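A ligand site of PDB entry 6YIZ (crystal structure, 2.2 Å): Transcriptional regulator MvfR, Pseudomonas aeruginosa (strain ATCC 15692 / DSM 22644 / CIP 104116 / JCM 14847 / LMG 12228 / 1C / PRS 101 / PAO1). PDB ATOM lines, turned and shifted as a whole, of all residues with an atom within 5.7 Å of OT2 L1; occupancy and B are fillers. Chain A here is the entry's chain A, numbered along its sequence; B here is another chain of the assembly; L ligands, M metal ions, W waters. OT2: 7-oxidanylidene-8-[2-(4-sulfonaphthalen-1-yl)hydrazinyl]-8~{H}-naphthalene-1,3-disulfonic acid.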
ATOM      1  N   PRO A  14      19.529  -4.588  30.129  1.00  0.00           N
ATOM      2  CA  PRO A  14      19.431  -5.389  31.347  1.00  0.00           C
ATOM      3  C   PRO A  14      20.026  -4.659  32.533  1.00  0.00           C
ATOM      4  O   PRO A  14      20.834  -3.727  32.373  1.00  0.00           O
ATOM      5  CB  PRO A  14      20.240  -6.641  31.022  1.00  0.00           C
ATOM      6  CG  PRO A  14      21.188  -6.195  30.114  1.00  0.00           C
ATOM      7  CD  PRO A  14      20.548  -5.123  29.241  1.00  0.00           C
ATOM      8  N   SER A  16      22.297  -5.054  34.985  1.00  0.00           N
ATOM      9  CA  SER A  16      23.741  -4.997  34.778  1.00  0.00           C
ATOM     10  C   SER A  16      24.245  -3.990  33.755  1.00  0.00           C
ATOM     11  O   SER A  16      25.352  -3.407  33.869  1.00  0.00           O
ATOM     12  CB  SER A  16      24.117  -6.448  34.386  1.00  0.00           C
ATOM     13  OG  SER A  16      25.252  -6.503  33.548  1.00  0.00           O
ATOM     14  N   PHE A  17      23.499  -3.870  32.673  1.00  0.00           N
ATOM     15  CA  PHE A  17      23.887  -2.897  31.650  1.00  0.00           C
ATOM     16  C   PHE A  17      23.556  -1.500  32.162  1.00  0.00           C
ATOM     17  O   PHE A  17      24.379  -0.587  32.086  1.00  0.00           O
ATOM     18  CB  PHE A  17      23.142  -3.240  30.361  1.00  0.00           C
ATOM     19  CG  PHE A  17      23.729  -2.637  29.088  1.00  0.00           C
ATOM     20  CD1 PHE A  17      23.821  -1.269  28.912  1.00  0.00           C
ATOM     21  CD2 PHE A  17      24.058  -3.475  28.043  1.00  0.00           C
ATOM     22  CE1 PHE A  17      24.291  -0.767  27.720  1.00  0.00           C
ATOM     23  CE2 PHE A  17      24.522  -2.986  26.886  1.00  0.00           C
ATOM     24  CZ  PHE A  17      24.667  -1.623  26.719  1.00  0.00           C
ATOM     25  N   LEU A  73      26.609   1.570  21.724  1.00  0.00           N
ATOM     26  CA  LEU A  73      27.185   1.496  23.061  1.00  0.00           C
ATOM     27  C   LEU A  73      27.545   0.077  23.449  1.00  0.00           C
ATOM     28  O   LEU A  73      28.566  -0.156  24.107  1.00  0.00           O
ATOM     29  CB  LEU A  73      26.202   2.080  24.067  1.00  0.00           C
ATOM     30  CG  LEU A  73      26.696   2.239  25.504  1.00  0.00           C
ATOM     31  CD1 LEU A  73      27.968   3.062  25.518  1.00  0.00           C
ATOM     32  CD2 LEU A  73      25.642   2.921  26.377  1.00  0.00           C
ATOM     33  N   GLY A  74      26.729  -0.912  23.068  1.00  0.00           N
ATOM     34  CA  GLY A  74      27.129  -2.292  23.240  1.00  0.00           C
ATOM     35  C   GLY A  74      26.043  -3.165  22.638  1.00  0.00           C
ATOM     36  O   GLY A  74      25.302  -2.675  21.752  1.00  0.00           O
ATOM     37  N   TYR A  75      25.907  -4.400  23.130  1.00  0.00           N
ATOM     38  CA  TYR A  75      25.044  -5.406  22.540  1.00  0.00           C
ATOM     39  C   TYR A  75      24.319  -6.106  23.659  1.00  0.00           C
ATOM     40  O   TYR A  75      24.722  -6.059  24.838  1.00  0.00           O
ATOM     41  CB  TYR A  75      25.820  -6.419  21.644  1.00  0.00           C
ATOM     42  CG  TYR A  75      26.750  -5.748  20.690  1.00  0.00           C
ATOM     43  CD1 TYR A  75      27.848  -5.045  21.185  1.00  0.00           C
ATOM     44  CD2 TYR A  75      26.569  -5.775  19.304  1.00  0.00           C
ATOM     45  CE1 TYR A  75      28.743  -4.356  20.337  1.00  0.00           C
ATOM     46  CE2 TYR A  75      27.458  -5.088  18.448  1.00  0.00           C
ATOM     47  CZ  TYR A  75      28.544  -4.359  19.001  1.00  0.00           C
ATOM     48  OH  TYR A  75      29.500  -3.677  18.275  1.00  0.00           O
ATOM     49  N   THR A  76      23.206  -6.714  23.302  1.00  0.00           N
ATOM     50  CA  THR A  76      22.368  -7.422  24.266  1.00  0.00           C
ATOM     51  C   THR A  76      21.590  -8.436  23.432  1.00  0.00           C
ATOM     52  O   THR A  76      21.552  -8.332  22.202  1.00  0.00           O
ATOM     53  CB  THR A  76      21.465  -6.472  25.018  1.00  0.00           C
ATOM     54  OG1 THR A  76      20.872  -7.143  26.124  1.00  0.00           O
ATOM     55  CG2 THR A  76      20.331  -6.016  24.181  1.00  0.00           C
ATOM     56  N   LYS A  77      20.985  -9.399  24.119  1.00  0.00           N
ATOM     57  CA  LYS A  77      20.551 -10.665  23.538  1.00  0.00           C
ATOM     58  C   LYS A  77      19.098 -10.876  23.906  1.00  0.00           C
ATOM     59  O   LYS A  77      18.734 -10.699  25.059  1.00  0.00           O
ATOM     60  CB  LYS A  77      21.355 -11.864  24.059  1.00  0.00           C
ATOM     61  CG  LYS A  77      22.840 -11.690  23.818  1.00  0.00           C
ATOM     62  CD  LYS A  77      23.412 -12.610  22.703  1.00  0.00           C
ATOM     63  CE  LYS A  77      24.730 -12.066  22.125  1.00  0.00           C
ATOM     64  NZ  LYS A  77      24.874 -12.244  20.628  1.00  0.00           N
ATOM     65  N   HIS A 149      16.777 -11.424  27.276  1.00  0.00           N
ATOM     66  CA  HIS A 149      17.343 -12.505  28.067  1.00  0.00           C
ATOM     67  C   HIS A 149      16.980 -12.349  29.531  1.00  0.00           C
ATOM     68  O   HIS A 149      16.337 -13.216  30.135  1.00  0.00           O
ATOM     69  CB  HIS A 149      18.844 -12.482  27.819  1.00  0.00           C
ATOM     70  CG  HIS A 149      19.666 -13.244  28.817  1.00  0.00           C
ATOM     71  ND1 HIS A 149      19.946 -14.575  28.680  1.00  0.00           N
ATOM     72  CD2 HIS A 149      20.326 -12.827  29.935  1.00  0.00           C
ATOM     73  CE1 HIS A 149      20.704 -14.970  29.678  1.00  0.00           C
ATOM     74  NE2 HIS A 149      20.955 -13.932  30.451  1.00  0.00           N
ATOM     75  N   TYR A 150      17.328 -11.224  30.121  1.00  0.00           N
ATOM     76  CA  TYR A 150      17.251 -11.160  31.574  1.00  0.00           C
ATOM     77  C   TYR A 150      15.839 -11.290  32.062  1.00  0.00           C
ATOM     78  O   TYR A 150      15.638 -11.650  33.232  1.00  0.00           O
ATOM     79  CB  TYR A 150      17.853  -9.873  32.072  1.00  0.00           C
ATOM     80  CG  TYR A 150      16.923  -8.707  32.053  1.00  0.00           C
ATOM     81  CD1 TYR A 150      16.842  -7.900  30.934  1.00  0.00           C
ATOM     82  CD2 TYR A 150      16.185  -8.378  33.159  1.00  0.00           C
ATOM     83  CE1 TYR A 150      15.979  -6.787  30.909  1.00  0.00           C
ATOM     84  CE2 TYR A 150      15.331  -7.274  33.155  1.00  0.00           C
ATOM     85  CZ  TYR A 150      15.244  -6.468  32.028  1.00  0.00           C
ATOM     86  OH  TYR A 150      14.417  -5.375  31.989  1.00  0.00           O
ATOM     87  N   ASP A 174      21.239 -11.239  18.795  1.00  0.00           N
ATOM     88  CA  ASP A 174      22.115 -10.172  19.241  1.00  0.00           C
ATOM     89  C   ASP A 174      21.511  -8.865  18.806  1.00  0.00           C
ATOM     90  O   ASP A 174      21.309  -8.685  17.606  1.00  0.00           O
ATOM     91  CB  ASP A 174      23.489 -10.341  18.637  1.00  0.00           C
ATOM     92  CG  ASP A 174      24.510  -9.373  19.233  1.00  0.00           C
ATOM     93  OD1 ASP A 174      24.991  -9.615  20.395  1.00  0.00           O
ATOM     94  OD2 ASP A 174      24.863  -8.399  18.520  1.00  0.00           O
ATOM     95  N   ARG A 199      31.794   1.634  27.332  1.00  0.00           N
ATOM     96  CA  ARG A 199      31.995   0.623  26.300  1.00  0.00           C
ATOM     97  C   ARG A 199      32.899  -0.463  26.818  1.00  0.00           C
ATOM     98  O   ARG A 199      32.661  -1.662  26.562  1.00  0.00           O
ATOM     99  CB  ARG A 199      32.631   1.229  25.051  1.00  0.00           C
ATOM    100  CG  ARG A 199      31.618   1.989  24.285  1.00  0.00           C
ATOM    101  CD  ARG A 199      32.187   2.708  23.109  1.00  0.00           C
ATOM    102  NE  ARG A 199      31.138   2.840  22.084  1.00  0.00           N
ATOM    103  CZ  ARG A 199      31.162   3.776  21.153  1.00  0.00           C
ATOM    104  NH1 ARG A 199      32.151   4.662  21.141  1.00  0.00           N
ATOM    105  NH2 ARG A 199      30.153   3.864  20.276  1.00  0.00           N
ATOM    106  N   LEU A 202      31.093  -2.560  29.578  1.00  0.00           N
ATOM    107  CA  LEU A 202      30.043  -3.381  28.987  1.00  0.00           C
ATOM    108  C   LEU A 202      30.673  -4.525  28.204  1.00  0.00           C
ATOM    109  O   LEU A 202      30.154  -5.647  28.172  1.00  0.00           O
ATOM    110  CB  LEU A 202      29.179  -2.520  28.084  1.00  0.00           C
ATOM    111  CG  LEU A 202      28.478  -1.440  28.888  1.00  0.00           C
ATOM    112  CD1 LEU A 202      27.813  -0.467  27.952  1.00  0.00           C
ATOM    113  CD2 LEU A 202      27.473  -2.090  29.783  1.00  0.00           C
ATOM    114  N   ARG A 203      31.804  -4.264  27.581  1.00  0.00           N
ATOM    115  CA  ARG A 203      32.543  -5.295  26.880  1.00  0.00           C
ATOM    116  C   ARG A 203      32.997  -6.383  27.836  1.00  0.00           C
ATOM    117  O   ARG A 203      32.848  -7.576  27.556  1.00  0.00           O
ATOM    118  CB  ARG A 203      33.716  -4.655  26.178  1.00  0.00           C
ATOM    119  CG  ARG A 203      34.547  -5.628  25.507  1.00  0.00           C
ATOM    120  CD  ARG A 203      35.691  -4.944  24.820  1.00  0.00           C
ATOM    121  NE  ARG A 203      36.622  -5.991  24.412  1.00  0.00           N
ATOM    122  CZ  ARG A 203      37.743  -5.784  23.743  1.00  0.00           C
ATOM    123  NH1 ARG A 203      38.076  -4.548  23.389  1.00  0.00           N
ATOM    124  NH2 ARG A 203      38.523  -6.817  23.434  1.00  0.00           N
ATOM    125  N   LEU A 205      31.802  -7.068  30.859  1.00  0.00           N
ATOM    126  CA  LEU A 205      30.639  -7.752  31.390  1.00  0.00           C
ATOM    127  C   LEU A 205      30.050  -8.747  30.403  1.00  0.00           C
ATOM    128  O   LEU A 205      29.445  -9.753  30.818  1.00  0.00           O
ATOM    129  CB  LEU A 205      29.606  -6.703  31.764  1.00  0.00           C
ATOM    130  CG  LEU A 205      28.695  -6.907  32.933  1.00  0.00           C
ATOM    131  CD1 LEU A 205      29.507  -7.355  34.137  1.00  0.00           C
ATOM    132  CD2 LEU A 205      28.006  -5.551  33.120  1.00  0.00           C
ATOM    133  N   GLY A 206      30.196  -8.504  29.118  1.00  0.00           N
ATOM    134  CA  GLY A 206      29.434  -9.237  28.142  1.00  0.00           C
ATOM    135  C   GLY A 206      30.222 -10.452  27.733  1.00  0.00           C
ATOM    136  O   GLY A 206      29.683 -11.567  27.636  1.00  0.00           O
ATOM    137  N   ARG A 207      31.513 -10.220  27.513  1.00  0.00           N
ATOM    138  CA  ARG A 207      32.437 -11.338  27.286  1.00  0.00           C
ATOM    139  C   ARG A 207      32.531 -12.259  28.500  1.00  0.00           C
ATOM    140  O   ARG A 207      32.878 -13.435  28.340  1.00  0.00           O
ATOM    141  CB  ARG A 207      33.824 -10.823  26.922  1.00  0.00           C
ATOM    142  CG  ARG A 207      33.867  -9.821  25.747  1.00  0.00           C
ATOM    143  CD  ARG A 207      33.630 -10.470  24.385  1.00  0.00           C
ATOM    144  NE  ARG A 207      33.920 -11.906  24.343  1.00  0.00           N
ATOM    145  CZ  ARG A 207      33.095 -12.842  23.864  1.00  0.00           C
ATOM    146  NH1 ARG A 207      33.499 -14.101  23.887  1.00  0.00           N
ATOM    147  NH2 ARG A 207      31.901 -12.550  23.328  1.00  0.00           N
ATOM    148  N   ARG A 209      30.317 -13.671  30.273  1.00  0.00           N
ATOM    149  CA  ARG A 209      29.369 -14.767  30.362  1.00  0.00           C
ATOM    150  C   ARG A 209      29.971 -16.097  29.923  1.00  0.00           C
ATOM    151  O   ARG A 209      29.442 -17.153  30.312  1.00  0.00           O
ATOM    152  CB  ARG A 209      28.152 -14.449  29.507  1.00  0.00           C
ATOM    153  CG  ARG A 209      27.517 -13.102  29.795  1.00  0.00           C
ATOM    154  CD  ARG A 209      26.554 -12.837  28.681  1.00  0.00           C
ATOM    155  NE  ARG A 209      27.288 -12.475  27.468  1.00  0.00           N
ATOM    156  CZ  ARG A 209      26.842 -12.637  26.218  1.00  0.00           C
ATOM    157  NH1 ARG A 209      25.659 -13.186  25.988  1.00  0.00           N
ATOM    158  NH2 ARG A 209      27.611 -12.261  25.198  1.00  0.00           N
ATOM    159  N   PHE A 210      31.057 -16.074  29.151  1.00  0.00           N
ATOM    160  CA  PHE A 210      31.675 -17.281  28.592  1.00  0.00           C
ATOM    161  C   PHE A 210      32.675 -17.957  29.524  1.00  0.00           C
ATOM    162  O   PHE A 210      33.196 -19.034  29.193  1.00  0.00           O
ATOM    163  CB  PHE A 210      32.326 -16.929  27.239  1.00  0.00           C
ATOM    164  CG  PHE A 210      31.348 -16.349  26.281  1.00  0.00           C
ATOM    165  CD1 PHE A 210      31.055 -14.997  26.304  1.00  0.00           C
ATOM    166  CD2 PHE A 210      30.657 -17.170  25.411  1.00  0.00           C
ATOM    167  CE1 PHE A 210      30.101 -14.446  25.453  1.00  0.00           C
ATOM    168  CE2 PHE A 210      29.692 -16.633  24.559  1.00  0.00           C
ATOM    169  CZ  PHE A 210      29.412 -15.277  24.583  1.00  0.00           C
ATOM    170  N   LYS B  77      32.490  -7.348  10.146  1.00  0.00           N
ATOM    171  CA  LYS B  77      32.824  -5.993  10.605  1.00  0.00           C
ATOM    172  C   LYS B  77      33.049  -5.103   9.392  1.00  0.00           C
ATOM    173  O   LYS B  77      33.782  -5.482   8.475  1.00  0.00           O
ATOM    174  CB  LYS B  77      34.073  -6.032  11.533  1.00  0.00           C
ATOM    175  CG  LYS B  77      33.827  -5.550  13.011  1.00  0.00           C
ATOM    176  CD  LYS B  77      33.046  -6.561  13.885  1.00  0.00           C
ATOM    177  CE  LYS B  77      32.578  -5.941  15.217  1.00  0.00           C
ATOM    178  NZ  LYS B  77      31.841  -6.917  16.060  1.00  0.00           N
ATOM    179  N   ARG B 207      36.796 -14.518  17.493  1.00  0.00           N
ATOM    180  CA  ARG B 207      37.425 -14.178  18.762  1.00  0.00           C
ATOM    181  C   ARG B 207      38.938 -14.124  18.630  1.00  0.00           C
ATOM    182  O   ARG B 207      39.590 -13.395  19.394  1.00  0.00           O
ATOM    183  CB  ARG B 207      37.026 -15.177  19.840  1.00  0.00           C
ATOM    184  CG  ARG B 207      35.552 -15.325  20.012  1.00  0.00           C
ATOM    185  CD  ARG B 207      34.853 -13.958  20.072  1.00  0.00           C
ATOM    186  NE  ARG B 207      35.425 -13.030  21.048  1.00  0.00           N
ATOM    187  CZ  ARG B 207      35.193 -11.712  21.079  1.00  0.00           C
ATOM    188  NH1 ARG B 207      35.768 -10.959  22.011  1.00  0.00           N
ATOM    189  NH2 ARG B 207      34.389 -11.136  20.187  1.00  0.00           N
ATOM    190  N   ARG B 209      40.806 -12.504  16.934  1.00  0.00           N
ATOM    191  CA  ARG B 209      41.388 -11.188  16.710  1.00  0.00           C
ATOM    192  C   ARG B 209      41.989 -10.574  17.969  1.00  0.00           C
ATOM    193  O   ARG B 209      42.660  -9.538  17.864  1.00  0.00           O
ATOM    194  CB  ARG B 209      40.301 -10.288  16.110  1.00  0.00           C
ATOM    195  CG  ARG B 209      39.653 -10.896  14.863  1.00  0.00           C
ATOM    196  CD  ARG B 209      38.402 -10.134  14.446  1.00  0.00           C
ATOM    197  NE  ARG B 209      37.309 -10.321  15.394  1.00  0.00           N
ATOM    198  CZ  ARG B 209      36.312  -9.466  15.647  1.00  0.00           C
ATOM    199  NH1 ARG B 209      36.244  -8.286  15.021  1.00  0.00           N
ATOM    200  NH2 ARG B 209      35.392  -9.778  16.541  1.00  0.00           N
ATOM    201  N   PHE B 210      41.797 -11.192  19.148  1.00  0.00           N
ATOM    202  CA  PHE B 210      42.311 -10.688  20.426  1.00  0.00           C
ATOM    203  C   PHE B 210      43.297 -11.661  21.088  1.00  0.00           C
ATOM    204  O   PHE B 210      44.529 -11.543  20.917  1.00  0.00           O
ATOM    205  CB  PHE B 210      41.138 -10.431  21.399  1.00  0.00           C
ATOM    206  CG  PHE B 210      39.950  -9.757  20.761  1.00  0.00           C
ATOM    207  CD1 PHE B 210      38.964 -10.506  20.114  1.00  0.00           C
ATOM    208  CD2 PHE B 210      39.807  -8.373  20.822  1.00  0.00           C
ATOM    209  CE1 PHE B 210      37.838  -9.878  19.512  1.00  0.00           C
ATOM    210  CE2 PHE B 210      38.704  -7.749  20.229  1.00  0.00           C
ATOM    211  CZ  PHE B 210      37.721  -8.506  19.567  1.00  0.00           C
HETATM  212  C05 OT2 L   1      32.713  -6.955  22.256  1.00  0.00           C
HETATM  213  C06 OT2 L   1      32.481  -5.650  22.677  1.00  0.00           C
HETATM  214  C07 OT2 L   1      31.278  -5.382  23.380  1.00  0.00           C
HETATM  215  C08 OT2 L   1      31.042  -4.037  23.810  1.00  0.00           C
HETATM  216  C09 OT2 L   1      29.898  -3.720  24.518  1.00  0.00           C
HETATM  217  C10 OT2 L   1      29.001  -4.756  24.803  1.00  0.00           C
HETATM  218  C12 OT2 L   1      29.222  -6.074  24.381  1.00  0.00           C
HETATM  219  C15 OT2 L   1      26.788  -7.779  26.433  1.00  0.00           C
HETATM  220  C16 OT2 L   1      26.347  -8.841  25.628  1.00  0.00           C
HETATM  221  C17 OT2 L   1      25.268  -9.611  26.038  1.00  0.00           C
HETATM  222  C18 OT2 L   1      24.631  -9.298  27.261  1.00  0.00           C
HETATM  223  C19 OT2 L   1      25.077  -8.203  28.068  1.00  0.00           C
HETATM  224  C20 OT2 L   1      24.442  -7.848  29.293  1.00  0.00           C
HETATM  225  C21 OT2 L   1      24.923  -6.794  30.079  1.00  0.00           C
HETATM  226  C22 OT2 L   1      26.024  -6.049  29.669  1.00  0.00           C
HETATM  227  C23 OT2 L   1      26.634  -6.370  28.458  1.00  0.00           C
HETATM  228  C24 OT2 L   1      26.141  -7.459  27.663  1.00  0.00           C
HETATM  229  C29 OT2 L   1      30.393  -6.403  23.653  1.00  0.00           C
HETATM  230  C30 OT2 L   1      30.699  -7.758  23.219  1.00  0.00           C
HETATM  231  C31 OT2 L   1      31.854  -8.009  22.500  1.00  0.00           C
HETATM  232  N13 OT2 L   1      28.355  -6.966  24.704  1.00  0.00           N
HETATM  233  N14 OT2 L   1      27.905  -6.947  26.057  1.00  0.00           N
HETATM  234  O01 OT2 L   1      35.089  -6.108  21.322  1.00  0.00           O
HETATM  235  O03 OT2 L   1      34.819  -8.479  22.148  1.00  0.00           O
HETATM  236  O04 OT2 L   1      33.896  -7.904  19.945  1.00  0.00           O
HETATM  237  O11 OT2 L   1      27.993  -4.552  25.421  1.00  0.00           O
HETATM  238  O26 OT2 L   1      22.631 -11.119  26.699  1.00  0.00           O
HETATM  239  O27 OT2 L   1      22.120  -9.147  28.067  1.00  0.00           O
HETATM  240  O28 OT2 L   1      23.217 -10.926  29.156  1.00  0.00           O
HETATM  241  O33 OT2 L   1      29.564  -9.776  24.869  1.00  0.00           O
HETATM  242  O34 OT2 L   1      28.220  -9.055  23.020  1.00  0.00           O
HETATM  243  O35 OT2 L   1      30.231 -10.203  22.351  1.00  0.00           O
HETATM  244  S02 OT2 L   1      34.192  -7.344  21.370  1.00  0.00           S
HETATM  245  S25 OT2 L   1      23.173 -10.215  27.800  1.00  0.00           S
HETATM  246  S32 OT2 L   1      29.655  -9.230  23.419  1.00  0.00           S
HETATM  247  C05 OT2 L   2      30.589 -14.975  19.164  1.00  0.00           C
HETATM  248  C06 OT2 L   2      30.156 -15.884  18.225  1.00  0.00           C
HETATM  249  C07 OT2 L   2      30.471 -15.712  16.839  1.00  0.00           C
HETATM  250  C08 OT2 L   2      29.999 -16.685  15.881  1.00  0.00           C
HETATM  251  C09 OT2 L   2      30.297 -16.540  14.528  1.00  0.00           C
HETATM  252  C10 OT2 L   2      31.081 -15.439  14.098  1.00  0.00           C
HETATM  253  C12 OT2 L   2      31.525 -14.496  15.046  1.00  0.00           C
HETATM  254  C15 OT2 L   2      33.829 -12.794  12.867  1.00  0.00           C
HETATM  255  C16 OT2 L   2      33.860 -11.465  13.324  1.00  0.00           C
HETATM  256  C17 OT2 L   2      34.548 -10.497  12.592  1.00  0.00           C
HETATM  257  C18 OT2 L   2      35.209 -10.877  11.416  1.00  0.00           C
HETATM  258  C19 OT2 L   2      35.163 -12.232  10.964  1.00  0.00           C
HETATM  259  C20 OT2 L   2      35.829 -12.620   9.746  1.00  0.00           C
HETATM  260  C21 OT2 L   2      35.807 -13.968   9.338  1.00  0.00           C
HETATM  261  C22 OT2 L   2      35.126 -14.935  10.078  1.00  0.00           C
HETATM  262  C23 OT2 L   2      34.464 -14.554  11.253  1.00  0.00           C
HETATM  263  C24 OT2 L   2      34.493 -13.184  11.691  1.00  0.00           C
HETATM  264  C29 OT2 L   2      31.223 -14.632  16.428  1.00  0.00           C
HETATM  265  C30 OT2 L   2      31.685 -13.684  17.413  1.00  0.00           C
HETATM  266  C31 OT2 L   2      31.349 -13.871  18.754  1.00  0.00           C
HETATM  267  N13 OT2 L   2      32.209 -13.529  14.612  1.00  0.00           N
HETATM  268  N14 OT2 L   2      33.146 -13.854  13.588  1.00  0.00           N
HETATM  269  O01 OT2 L   2      31.535 -14.938  21.668  1.00  0.00           O
HETATM  270  O03 OT2 L   2      29.191 -14.106  21.396  1.00  0.00           O
HETATM  271  O04 OT2 L   2      29.516 -16.487  21.211  1.00  0.00           O
HETATM  272  O11 OT2 L   2      31.377 -15.281  12.930  1.00  0.00           O
HETATM  273  O26 OT2 L   2      36.055  -8.259  11.057  1.00  0.00           O
HETATM  274  O27 OT2 L   2      35.171  -9.653   9.142  1.00  0.00           O
HETATM  275  O28 OT2 L   2      37.414 -10.019   9.892  1.00  0.00           O
HETATM  276  O33 OT2 L   2      34.135 -12.250  17.007  1.00  0.00           O
HETATM  277  O34 OT2 L   2      32.050 -11.247  16.077  1.00  0.00           O
HETATM  278  O35 OT2 L   2      32.255 -11.392  18.427  1.00  0.00           O
HETATM  279  S02 OT2 L   2      30.209 -15.157  20.929  1.00  0.00           S
HETATM  280  S25 OT2 L   2      36.029  -9.642  10.407  1.00  0.00           S
HETATM  281  S32 OT2 L   2      32.611 -12.172  17.159  1.00  0.00           S
HETATM  282 MG    MG M   1      28.868  -9.569  18.605  1.00  0.00          MG
HETATM  283  O   HOH W   1      27.724  -9.394  20.397  1.00  0.00           O
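N of Tyr 75 is in hydrogen-bond range of O11 of OT2 L1, at 3.1 Å.
O27 of OT2 L1 sits at hydrogen-bond distance from OG1 of Thr 76, 3.1 Å away.
NH1 of Arg 207 of chain B is in salt-bridge range of O03 of OT2 L1.
O33 of OT2 L2 lies within salt-bridge range of NH2 of Arg 209 of chain B, at 2.8 Å.
NH2 of Arg 207 of chain A is in salt-bridge range of O01 of OT2 L2 (2.9 Å).
NH2 of Arg 207 of chain A is in salt-bridge range of O35 of OT2 L1 (3.0 Å).
The backbone NH of Arg 207 of chain A lies within hydrogen-bond range of an oxygen (O33) of OT2 L1 (3.3 Å).
NE of Arg 203 is in salt-bridge range of O01 of OT2 L1 (3.5 Å).
O of Leu 202 sits at hydrogen-bond distance from N14 of OT2 L1 (3.3 Å).
NH2 of Arg 209 of chain A lies within salt-bridge range of O33 of OT2 L1 (3.2 Å).
O35 of OT2 L2 is in salt-bridge range of NH2 of Arg 207 of chain B, at 2.8 Å.
The backbone carbonyl oxygen (O) of Gly 206 sits at hydrogen-bond distance from the guanidinium group (NE) of Arg 209 of chain A (2.6 Å).
The backbone carbonyl oxygen (O) of Lys 77 of chain A lies within hydrogen-bond range of the backbone NH (N) of His 149 (3.0 Å).
The side-chain carboxylate (OD1) of Asp 174 is in salt-bridge range of the side-chain amino group (NZ) of Lys 77 of chain A (2.6 Å).
The backbone carbonyl oxygen of Gly 206 lies close to an oxygen (O33) of OT2 L1, 3.3 Å away.
Pro 14 touches OT2 L1 (CG to O27, 3.7 Å).
Ser 16 touches OT2 L1 (OG to C21, 3.5 Å).
Phe 17 touches OT2 L1 (CD2 to C22, 3.6 Å).
Leu 73 touches OT2 L1 (O to C09, 3.8 Å).
Gly 74 touches OT2 L1 (CA to O11, 3.3 Å).
Lys 77 of chain A touches OT2 L1.
His 149 touches OT2 L1.
Arg 199 touches OT2 L1 (O to C08, 3.98 Å).
Phe 210 of chain B touches OT2 L1.
Hydrophobic or aromatic side chains that line OT2 L1: Pro 14, Phe 17, Tyr 75, His 149, Leu 202 and Phe 210 of chain B.
The nearest printed residue that does not touch OT2 L1 is Leu 205 (4.01 Å).
Water W1 lies within hydrogen-bond range of an oxygen (O34) of OT2 L1 (2.7 Å) and the side-chain carboxylate of Asp 174 (2.7 Å).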
